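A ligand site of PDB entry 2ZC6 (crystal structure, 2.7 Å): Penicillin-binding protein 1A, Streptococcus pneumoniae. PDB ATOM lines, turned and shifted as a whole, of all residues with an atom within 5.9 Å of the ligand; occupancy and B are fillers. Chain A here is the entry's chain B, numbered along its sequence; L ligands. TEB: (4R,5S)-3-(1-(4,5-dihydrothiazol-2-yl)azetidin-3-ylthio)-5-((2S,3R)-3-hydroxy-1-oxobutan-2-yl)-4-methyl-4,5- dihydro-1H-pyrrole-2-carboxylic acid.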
ATOM      1  N   TRP A 105     -29.399  17.927 -23.817  1.00  0.00           N
ATOM      2  CA  TRP A 105     -29.604  17.726 -22.388  1.00  0.00           C
ATOM      3  C   TRP A 105     -29.657  16.252 -21.956  1.00  0.00           C
ATOM      4  O   TRP A 105     -29.872  15.968 -20.776  1.00  0.00           O
ATOM      5  CB  TRP A 105     -30.807  18.511 -21.896  1.00  0.00           C
ATOM      6  CG  TRP A 105     -30.410  19.902 -21.543  1.00  0.00           C
ATOM      7  CD1 TRP A 105     -30.186  20.930 -22.396  1.00  0.00           C
ATOM      8  CD2 TRP A 105     -30.153  20.406 -20.232  1.00  0.00           C
ATOM      9  NE1 TRP A 105     -29.816  22.051 -21.698  1.00  0.00           N
ATOM     10  CE2 TRP A 105     -29.785  21.753 -20.369  1.00  0.00           C
ATOM     11  CE3 TRP A 105     -30.193  19.841 -18.945  1.00  0.00           C
ATOM     12  CZ2 TRP A 105     -29.464  22.556 -19.268  1.00  0.00           C
ATOM     13  CZ3 TRP A 105     -29.869  20.637 -17.855  1.00  0.00           C
ATOM     14  CH2 TRP A 105     -29.516  21.979 -18.027  1.00  0.00           C
ATOM     15  N   GLY A 106     -29.450  15.346 -22.910  1.00  0.00           N
ATOM     16  CA  GLY A 106     -29.301  13.915 -22.632  1.00  0.00           C
ATOM     17  C   GLY A 106     -30.308  13.302 -21.683  1.00  0.00           C
ATOM     18  O   GLY A 106     -31.524  13.403 -21.887  1.00  0.00           O
ATOM     19  N   SER A 107     -29.803  12.689 -20.616  1.00  0.00           N
ATOM     20  CA  SER A 107     -30.618  11.880 -19.693  1.00  0.00           C
ATOM     21  C   SER A 107     -31.577  12.692 -18.816  1.00  0.00           C
ATOM     22  O   SER A 107     -32.480  12.119 -18.187  1.00  0.00           O
ATOM     23  CB  SER A 107     -29.774  10.936 -18.804  1.00  0.00           C
ATOM     24  OG  SER A 107     -28.954   9.985 -19.555  1.00  0.00           O
ATOM     25  N   THR A 108     -31.397  14.002 -18.766  1.00  0.00           N
ATOM     26  CA  THR A 108     -32.306  14.858 -17.996  1.00  0.00           C
ATOM     27  C   THR A 108     -33.694  14.918 -18.644  1.00  0.00           C
ATOM     28  O   THR A 108     -34.669  15.322 -18.013  1.00  0.00           O
ATOM     29  CB  THR A 108     -31.734  16.273 -17.732  1.00  0.00           C
ATOM     30  OG1 THR A 108     -31.283  16.848 -18.970  1.00  0.00           O
ATOM     31  CG2 THR A 108     -30.579  16.234 -16.731  1.00  0.00           C
ATOM     32  N   LYS A 110     -35.231  12.167 -19.561  1.00  0.00           N
ATOM     33  CA  LYS A 110     -35.932  10.947 -19.129  1.00  0.00           C
ATOM     34  C   LYS A 110     -37.111  11.165 -18.173  1.00  0.00           C
ATOM     35  O   LYS A 110     -38.218  10.703 -18.472  1.00  0.00           O
ATOM     36  CB  LYS A 110     -34.974   9.905 -18.541  1.00  0.00           C
ATOM     37  CG  LYS A 110     -34.128   9.164 -19.559  1.00  0.00           C
ATOM     38  CD  LYS A 110     -33.218   8.181 -18.858  1.00  0.00           C
ATOM     39  CE  LYS A 110     -31.893   8.022 -19.566  1.00  0.00           C
ATOM     40  NZ  LYS A 110     -31.015   7.018 -18.895  1.00  0.00           N
ATOM     41  N   TYR A 146     -28.130   1.318 -26.869  1.00  0.00           N
ATOM     42  CA  TYR A 146     -27.052   0.885 -25.994  1.00  0.00           C
ATOM     43  C   TYR A 146     -27.120   1.574 -24.643  1.00  0.00           C
ATOM     44  O   TYR A 146     -27.514   2.727 -24.551  1.00  0.00           O
ATOM     45  CB  TYR A 146     -25.696   1.158 -26.645  1.00  0.00           C
ATOM     46  CG  TYR A 146     -25.400   0.354 -27.885  1.00  0.00           C
ATOM     47  CD1 TYR A 146     -25.273   0.969 -29.129  1.00  0.00           C
ATOM     48  CD2 TYR A 146     -25.247  -1.040 -27.815  1.00  0.00           C
ATOM     49  CE1 TYR A 146     -24.994   0.234 -30.271  1.00  0.00           C
ATOM     50  CE2 TYR A 146     -24.966  -1.784 -28.959  1.00  0.00           C
ATOM     51  CZ  TYR A 146     -24.845  -1.143 -30.187  1.00  0.00           C
ATOM     52  OH  TYR A 146     -24.578  -1.884 -31.311  1.00  0.00           O
ATOM     53  N   ASN A 147     -26.738   0.856 -23.595  1.00  0.00           N
ATOM     54  CA  ASN A 147     -26.457   1.500 -22.330  1.00  0.00           C
ATOM     55  C   ASN A 147     -25.039   2.055 -22.356  1.00  0.00           C
ATOM     56  O   ASN A 147     -24.261   1.722 -23.251  1.00  0.00           O
ATOM     57  CB  ASN A 147     -26.654   0.525 -21.171  1.00  0.00           C
ATOM     58  CG  ASN A 147     -28.117   0.285 -20.865  1.00  0.00           C
ATOM     59  OD1 ASN A 147     -28.880   1.239 -20.687  1.00  0.00           O
ATOM     60  ND2 ASN A 147     -28.517  -0.977 -20.814  1.00  0.00           N
ATOM     61  N   TRP A 148     -24.707   2.910 -21.385  1.00  0.00           N
ATOM     62  CA  TRP A 148     -23.383   3.535 -21.343  1.00  0.00           C
ATOM     63  C   TRP A 148     -22.260   2.510 -21.250  1.00  0.00           C
ATOM     64  O   TRP A 148     -21.204   2.689 -21.844  1.00  0.00           O
ATOM     65  CB  TRP A 148     -23.290   4.553 -20.194  1.00  0.00           C
ATOM     66  CG  TRP A 148     -23.170   3.978 -18.809  1.00  0.00           C
ATOM     67  CD1 TRP A 148     -24.192   3.665 -17.954  1.00  0.00           C
ATOM     68  CD2 TRP A 148     -21.961   3.664 -18.119  1.00  0.00           C
ATOM     69  NE1 TRP A 148     -23.692   3.162 -16.778  1.00  0.00           N
ATOM     70  CE2 TRP A 148     -22.326   3.151 -16.845  1.00  0.00           C
ATOM     71  CE3 TRP A 148     -20.593   3.752 -18.441  1.00  0.00           C
ATOM     72  CZ2 TRP A 148     -21.373   2.731 -15.909  1.00  0.00           C
ATOM     73  CZ3 TRP A 148     -19.649   3.330 -17.506  1.00  0.00           C
ATOM     74  CH2 TRP A 148     -20.053   2.825 -16.256  1.00  0.00           C
ATOM     75  N   GLN A 163     -32.545   5.620 -11.528  1.00  0.00           N
ATOM     76  CA  GLN A 163     -31.430   5.907 -10.619  1.00  0.00           C
ATOM     77  C   GLN A 163     -30.072   5.615 -11.262  1.00  0.00           C
ATOM     78  O   GLN A 163     -29.154   6.420 -11.180  1.00  0.00           O
ATOM     79  CB  GLN A 163     -31.639   5.118  -9.323  1.00  0.00           C
ATOM     80  CG  GLN A 163     -30.430   4.928  -8.436  1.00  0.00           C
ATOM     81  CD  GLN A 163     -30.677   3.862  -7.388  1.00  0.00           C
ATOM     82  OE1 GLN A 163     -29.832   2.987  -7.186  1.00  0.00           O
ATOM     83  NE2 GLN A 163     -31.825   3.921  -6.726  1.00  0.00           N
ATOM     84  N   GLN A 164     -29.961   4.454 -11.906  1.00  0.00           N
ATOM     85  CA  GLN A 164     -28.750   4.077 -12.629  1.00  0.00           C
ATOM     86  C   GLN A 164     -28.675   4.701 -14.011  1.00  0.00           C
ATOM     87  O   GLN A 164     -27.643   4.610 -14.683  1.00  0.00           O
ATOM     88  CB  GLN A 164     -28.660   2.554 -12.742  1.00  0.00           C
ATOM     89  CG  GLN A 164     -28.327   1.882 -11.429  1.00  0.00           C
ATOM     90  CD  GLN A 164     -27.101   2.479 -10.783  1.00  0.00           C
ATOM     91  OE1 GLN A 164     -25.982   2.300 -11.261  1.00  0.00           O
ATOM     92  NE2 GLN A 164     -27.302   3.206  -9.676  1.00  0.00           N
ATOM     93  N   SER A 165     -29.777   5.338 -14.413  1.00  0.00           N
ATOM     94  CA  SER A 165     -29.915   5.994 -15.708  1.00  0.00           C
ATOM     95  C   SER A 165     -29.677   5.038 -16.878  1.00  0.00           C
ATOM     96  O   SER A 165     -28.777   5.243 -17.690  1.00  0.00           O
ATOM     97  CB  SER A 165     -29.006   7.205 -15.818  1.00  0.00           C
ATOM     98  OG  SER A 165     -29.427   8.042 -16.872  1.00  0.00           O
ATOM     99  N   ASN A 167     -30.733   3.216 -20.423  1.00  0.00           N
ATOM    100  CA  ASN A 167     -31.345   3.744 -21.626  1.00  0.00           C
ATOM    101  C   ASN A 167     -32.497   2.922 -22.173  1.00  0.00           C
ATOM    102  O   ASN A 167     -33.550   3.463 -22.521  1.00  0.00           O
ATOM    103  CB  ASN A 167     -30.292   4.022 -22.714  1.00  0.00           C
ATOM    104  CG  ASN A 167     -29.505   5.312 -22.445  1.00  0.00           C
ATOM    105  OD1 ASN A 167     -29.934   6.184 -21.680  1.00  0.00           O
ATOM    106  ND2 ASN A 167     -28.350   5.440 -23.092  1.00  0.00           N
ATOM    107  N   ILE A 202     -33.931   9.923 -24.694  1.00  0.00           N
ATOM    108  CA  ILE A 202     -32.637  10.115 -24.047  1.00  0.00           C
ATOM    109  C   ILE A 202     -31.861  11.316 -24.609  1.00  0.00           C
ATOM    110  O   ILE A 202     -30.632  11.392 -24.484  1.00  0.00           O
ATOM    111  CB  ILE A 202     -31.784   8.816 -24.092  1.00  0.00           C
ATOM    112  CG1 ILE A 202     -31.518   8.378 -25.547  1.00  0.00           C
ATOM    113  CG2 ILE A 202     -32.468   7.706 -23.290  1.00  0.00           C
ATOM    114  CD1 ILE A 202     -30.371   7.396 -25.720  1.00  0.00           C
ATOM    115  N   THR A 280     -26.411   8.122  -9.743  1.00  0.00           N
ATOM    116  CA  THR A 280     -25.444   8.878 -10.527  1.00  0.00           C
ATOM    117  C   THR A 280     -25.268  10.324 -10.061  1.00  0.00           C
ATOM    118  O   THR A 280     -24.388  11.030 -10.556  1.00  0.00           O
ATOM    119  CB  THR A 280     -25.838   8.917 -12.011  1.00  0.00           C
ATOM    120  OG1 THR A 280     -27.236   9.210 -12.117  1.00  0.00           O
ATOM    121  CG2 THR A 280     -25.582   7.568 -12.664  1.00  0.00           C
ATOM    122  N   LYS A 294     -31.762  14.806 -11.456  1.00  0.00           N
ATOM    123  CA  LYS A 294     -31.322  13.870 -12.484  1.00  0.00           C
ATOM    124  C   LYS A 294     -30.044  14.369 -13.140  1.00  0.00           C
ATOM    125  O   LYS A 294     -29.909  15.552 -13.458  1.00  0.00           O
ATOM    126  CB  LYS A 294     -32.434  13.674 -13.516  1.00  0.00           C
ATOM    127  CG  LYS A 294     -32.080  12.802 -14.724  1.00  0.00           C
ATOM    128  CD  LYS A 294     -32.404  11.325 -14.531  1.00  0.00           C
ATOM    129  CE  LYS A 294     -31.161  10.490 -14.285  1.00  0.00           C
ATOM    130  NZ  LYS A 294     -30.353  10.341 -15.514  1.00  0.00           N
ATOM    131  N   THR A 295     -29.092  13.455 -13.329  1.00  0.00           N
ATOM    132  CA  THR A 295     -27.852  13.752 -14.049  1.00  0.00           C
ATOM    133  C   THR A 295     -28.036  13.535 -15.552  1.00  0.00           C
ATOM    134  O   THR A 295     -29.059  13.033 -16.017  1.00  0.00           O
ATOM    135  CB  THR A 295     -26.686  12.861 -13.577  1.00  0.00           C
ATOM    136  OG1 THR A 295     -27.121  11.509 -13.531  1.00  0.00           O
ATOM    137  CG2 THR A 295     -26.189  13.285 -12.206  1.00  0.00           C
ATOM    138  N   GLY A 296     -27.025  13.938 -16.303  1.00  0.00           N
ATOM    139  CA  GLY A 296     -27.050  13.826 -17.752  1.00  0.00           C
ATOM    140  C   GLY A 296     -25.663  13.912 -18.331  1.00  0.00           C
ATOM    141  O   GLY A 296     -24.880  14.801 -17.996  1.00  0.00           O
ATOM    142  N   THR A 297     -25.359  12.980 -19.218  1.00  0.00           N
ATOM    143  CA  THR A 297     -24.106  12.968 -19.951  1.00  0.00           C
ATOM    144  C   THR A 297     -24.456  12.654 -21.402  1.00  0.00           C
ATOM    145  O   THR A 297     -24.765  11.504 -21.728  1.00  0.00           O
ATOM    146  CB  THR A 297     -23.128  11.929 -19.359  1.00  0.00           C
ATOM    147  OG1 THR A 297     -22.821  12.275 -17.998  1.00  0.00           O
ATOM    148  CG2 THR A 297     -21.830  11.874 -20.138  1.00  0.00           C
ATOM    149  N   SER A 298     -24.446  13.669 -22.251  1.00  0.00           N
ATOM    150  CA  SER A 298     -24.664  13.473 -23.690  1.00  0.00           C
ATOM    151  C   SER A 298     -23.446  12.783 -24.312  1.00  0.00           C
ATOM    152  O   SER A 298     -22.418  12.609 -23.670  1.00  0.00           O
ATOM    153  CB  SER A 298     -24.945  14.803 -24.391  1.00  0.00           C
ATOM    154  OG  SER A 298     -23.771  15.563 -24.529  1.00  0.00           O
ATOM    155  N   ASN A 299     -23.574  12.378 -25.574  1.00  0.00           N
ATOM    156  CA  ASN A 299     -22.472  11.699 -26.259  1.00  0.00           C
ATOM    157  C   ASN A 299     -22.261  12.174 -27.693  1.00  0.00           C
ATOM    158  O   ASN A 299     -23.115  12.838 -28.269  1.00  0.00           O
ATOM    159  CB  ASN A 299     -22.664  10.188 -26.214  1.00  0.00           C
ATOM    160  CG  ASN A 299     -24.038   9.776 -26.697  1.00  0.00           C
ATOM    161  OD1 ASN A 299     -24.259   9.621 -27.898  1.00  0.00           O
ATOM    162  ND2 ASN A 299     -24.962   9.601 -25.766  1.00  0.00           N
ATOM    163  N   PHE A 314     -13.602   7.889 -20.903  1.00  0.00           N
ATOM    164  CA  PHE A 314     -14.974   8.356 -20.829  1.00  0.00           C
ATOM    165  C   PHE A 314     -15.007   9.866 -21.075  1.00  0.00           C
ATOM    166  O   PHE A 314     -14.424  10.640 -20.313  1.00  0.00           O
ATOM    167  CB  PHE A 314     -15.567   8.018 -19.466  1.00  0.00           C
ATOM    168  CG  PHE A 314     -17.062   8.031 -19.434  1.00  0.00           C
ATOM    169  CD1 PHE A 314     -17.787   6.882 -19.723  1.00  0.00           C
ATOM    170  CD2 PHE A 314     -17.761   9.192 -19.094  1.00  0.00           C
ATOM    171  CE1 PHE A 314     -19.176   6.873 -19.684  1.00  0.00           C
ATOM    172  CE2 PHE A 314     -19.144   9.206 -19.060  1.00  0.00           C
ATOM    173  CZ  PHE A 314     -19.856   8.040 -19.351  1.00  0.00           C
ATOM    174  N   GLU A 319     -22.255  17.787 -19.882  1.00  0.00           N
ATOM    175  CA  GLU A 319     -22.598  17.193 -18.595  1.00  0.00           C
ATOM    176  C   GLU A 319     -23.689  18.071 -17.996  1.00  0.00           C
ATOM    177  O   GLU A 319     -23.592  19.290 -18.039  1.00  0.00           O
ATOM    178  CB  GLU A 319     -21.365  17.149 -17.691  1.00  0.00           C
ATOM    179  CG  GLU A 319     -21.623  16.706 -16.254  1.00  0.00           C
ATOM    180  CD  GLU A 319     -22.144  15.287 -16.172  1.00  0.00           C
ATOM    181  OE1 GLU A 319     -21.576  14.398 -16.823  1.00  0.00           O
ATOM    182  OE2 GLU A 319     -23.135  15.079 -15.433  1.00  0.00           O
ATOM    183  N   LEU A 320     -24.723  17.437 -17.449  1.00  0.00           N
ATOM    184  CA  LEU A 320     -25.944  18.150 -17.028  1.00  0.00           C
ATOM    185  C   LEU A 320     -26.499  17.682 -15.703  1.00  0.00           C
ATOM    186  O   LEU A 320     -26.517  16.483 -15.397  1.00  0.00           O
ATOM    187  CB  LEU A 320     -27.046  17.982 -18.083  1.00  0.00           C
ATOM    188  CG  LEU A 320     -26.525  18.081 -19.513  1.00  0.00           C
ATOM    189  CD1 LEU A 320     -26.881  16.822 -20.284  1.00  0.00           C
ATOM    190  CD2 LEU A 320     -26.996  19.358 -20.196  1.00  0.00           C
HETATM  191  C7  TEB L   1     -27.716  10.345 -20.001  1.00  0.00           C
HETATM  192  O14 TEB L   1     -27.365  11.504 -19.959  1.00  0.00           O
HETATM  193  C6  TEB L   1     -26.898   9.210 -20.539  1.00  0.00           C
HETATM  194  C8  TEB L   1     -27.580   8.631 -21.802  1.00  0.00           C
HETATM  195  O15 TEB L   1     -26.721   7.566 -22.287  1.00  0.00           O
HETATM  196  C9  TEB L   1     -27.777   9.653 -22.921  1.00  0.00           C
HETATM  197  C5  TEB L   1     -26.575   8.175 -19.430  1.00  0.00           C
HETATM  198  C1  TEB L   1     -25.058   7.738 -19.273  1.00  0.00           C
HETATM  199  C10 TEB L   1     -24.099   8.096 -20.435  1.00  0.00           C
HETATM  200  N4  TEB L   1     -26.869   8.708 -18.100  1.00  0.00           N
HETATM  201  C3  TEB L   1     -25.706   9.047 -17.432  1.00  0.00           C
HETATM  202  C11 TEB L   1     -25.866   9.962 -16.191  1.00  0.00           C
HETATM  203  O13 TEB L   1     -26.839   9.620 -15.493  1.00  0.00           O
HETATM  204  O12 TEB L   1     -25.055  10.892 -16.018  1.00  0.00           O
HETATM  205  C2  TEB L   1     -24.645   8.500 -17.995  1.00  0.00           C
HETATM  206  S16 TEB L   1     -23.029   8.627 -17.369  1.00  0.00           S
HETATM  207  C17 TEB L   1     -22.703   6.975 -16.731  1.00  0.00           C
HETATM  208  C20 TEB L   1     -23.364   6.550 -15.366  1.00  0.00           C
HETATM  209  N19 TEB L   1     -21.990   6.413 -14.810  1.00  0.00           N
HETATM  210  C18 TEB L   1     -21.308   6.933 -16.015  1.00  0.00           C
HETATM  211  C21 TEB L   1     -21.430   5.723 -13.819  1.00  0.00           C
HETATM  212  N25 TEB L   1     -20.221   5.798 -13.427  1.00  0.00           N
HETATM  213  C24 TEB L   1     -19.884   4.908 -12.301  1.00  0.00           C
HETATM  214  C23 TEB L   1     -21.066   3.923 -12.001  1.00  0.00           C
HETATM  215  S22 TEB L   1     -22.497   4.560 -12.938  1.00  0.00           S
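Gly 106 touches the ligand (C to O14, 3.9 Å).
CB of Trp 148 touches C10 of the ligand, at 3.6 Å.
Ile 202 touches the ligand (O to C9, 3.7 Å).
CA of Gly 296 touches O14 of the ligand, 3.2 Å away.
Phe 314 touches the ligand (CZ to S16, 3.8 Å).
Of the 23 residues printed, 12 come within 4 Å of the ligand.
OG1 of Thr 295 lies within hydrogen-bond range of OG1 of Thr 280 (2.7 Å).
O of Gly 296 is in hydrogen-bond range of N of Leu 320 (2.7 Å).
The side-chain amide oxygen of Asn 167 lies within hydrogen-bond range of the side-chain amino group of Lys 110 (3.1 Å).
The side-chain hydroxyl (OG) of Ser 165 lies within hydrogen-bond range of the side-chain amino group (NZ) of Lys 294 (2.8 Å).
N of Asn 167 lies within hydrogen-bond range of OD1 of Asn 147 (2.7 Å).
OG of Ser 107 is in hydrogen-bond range of OG of Ser 165.
OG of Ser 165 sits at hydrogen-bond distance from NZ of Lys 110, at 2.8 Å.
The backbone carbonyl oxygen of Tyr 146 sits at hydrogen-bond distance from the side-chain amide nitrogen of Asn 167 (3.2 Å).
OG of Ser 165 lies within hydrogen-bond range of N4 of the ligand (2.9 Å).
The side-chain hydroxyl of Thr 295 lies within hydrogen-bond range of an oxygen (O13) of the ligand (2.7 Å).
The side-chain hydroxyl (OG1) of Thr 297 lies within hydrogen-bond range of an oxygen (O12) of the ligand (3.3 Å).
O13 of the ligand sits at hydrogen-bond distance from OG1 of Thr 280, 3.4 Å away.
An oxygen (O14) of the ligand lies within hydrogen-bond range of the backbone NH (N) of Thr 297 (2.6 Å).
O15 of the ligand lies within hydrogen-bond range of ND2 of Asn 167 (2.8 Å).
A carbon (C7) of the ligand is bonded to the side-chain hydroxyl (OG) of Ser 107, at 1.4 Å.
The backbone NH (N) of Ser 107 lies close to an oxygen (O14) of the ligand, 2.8 Å away.
O13 of the ligand lies within salt-bridge range of NZ of Lys 294 (3.6 Å).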
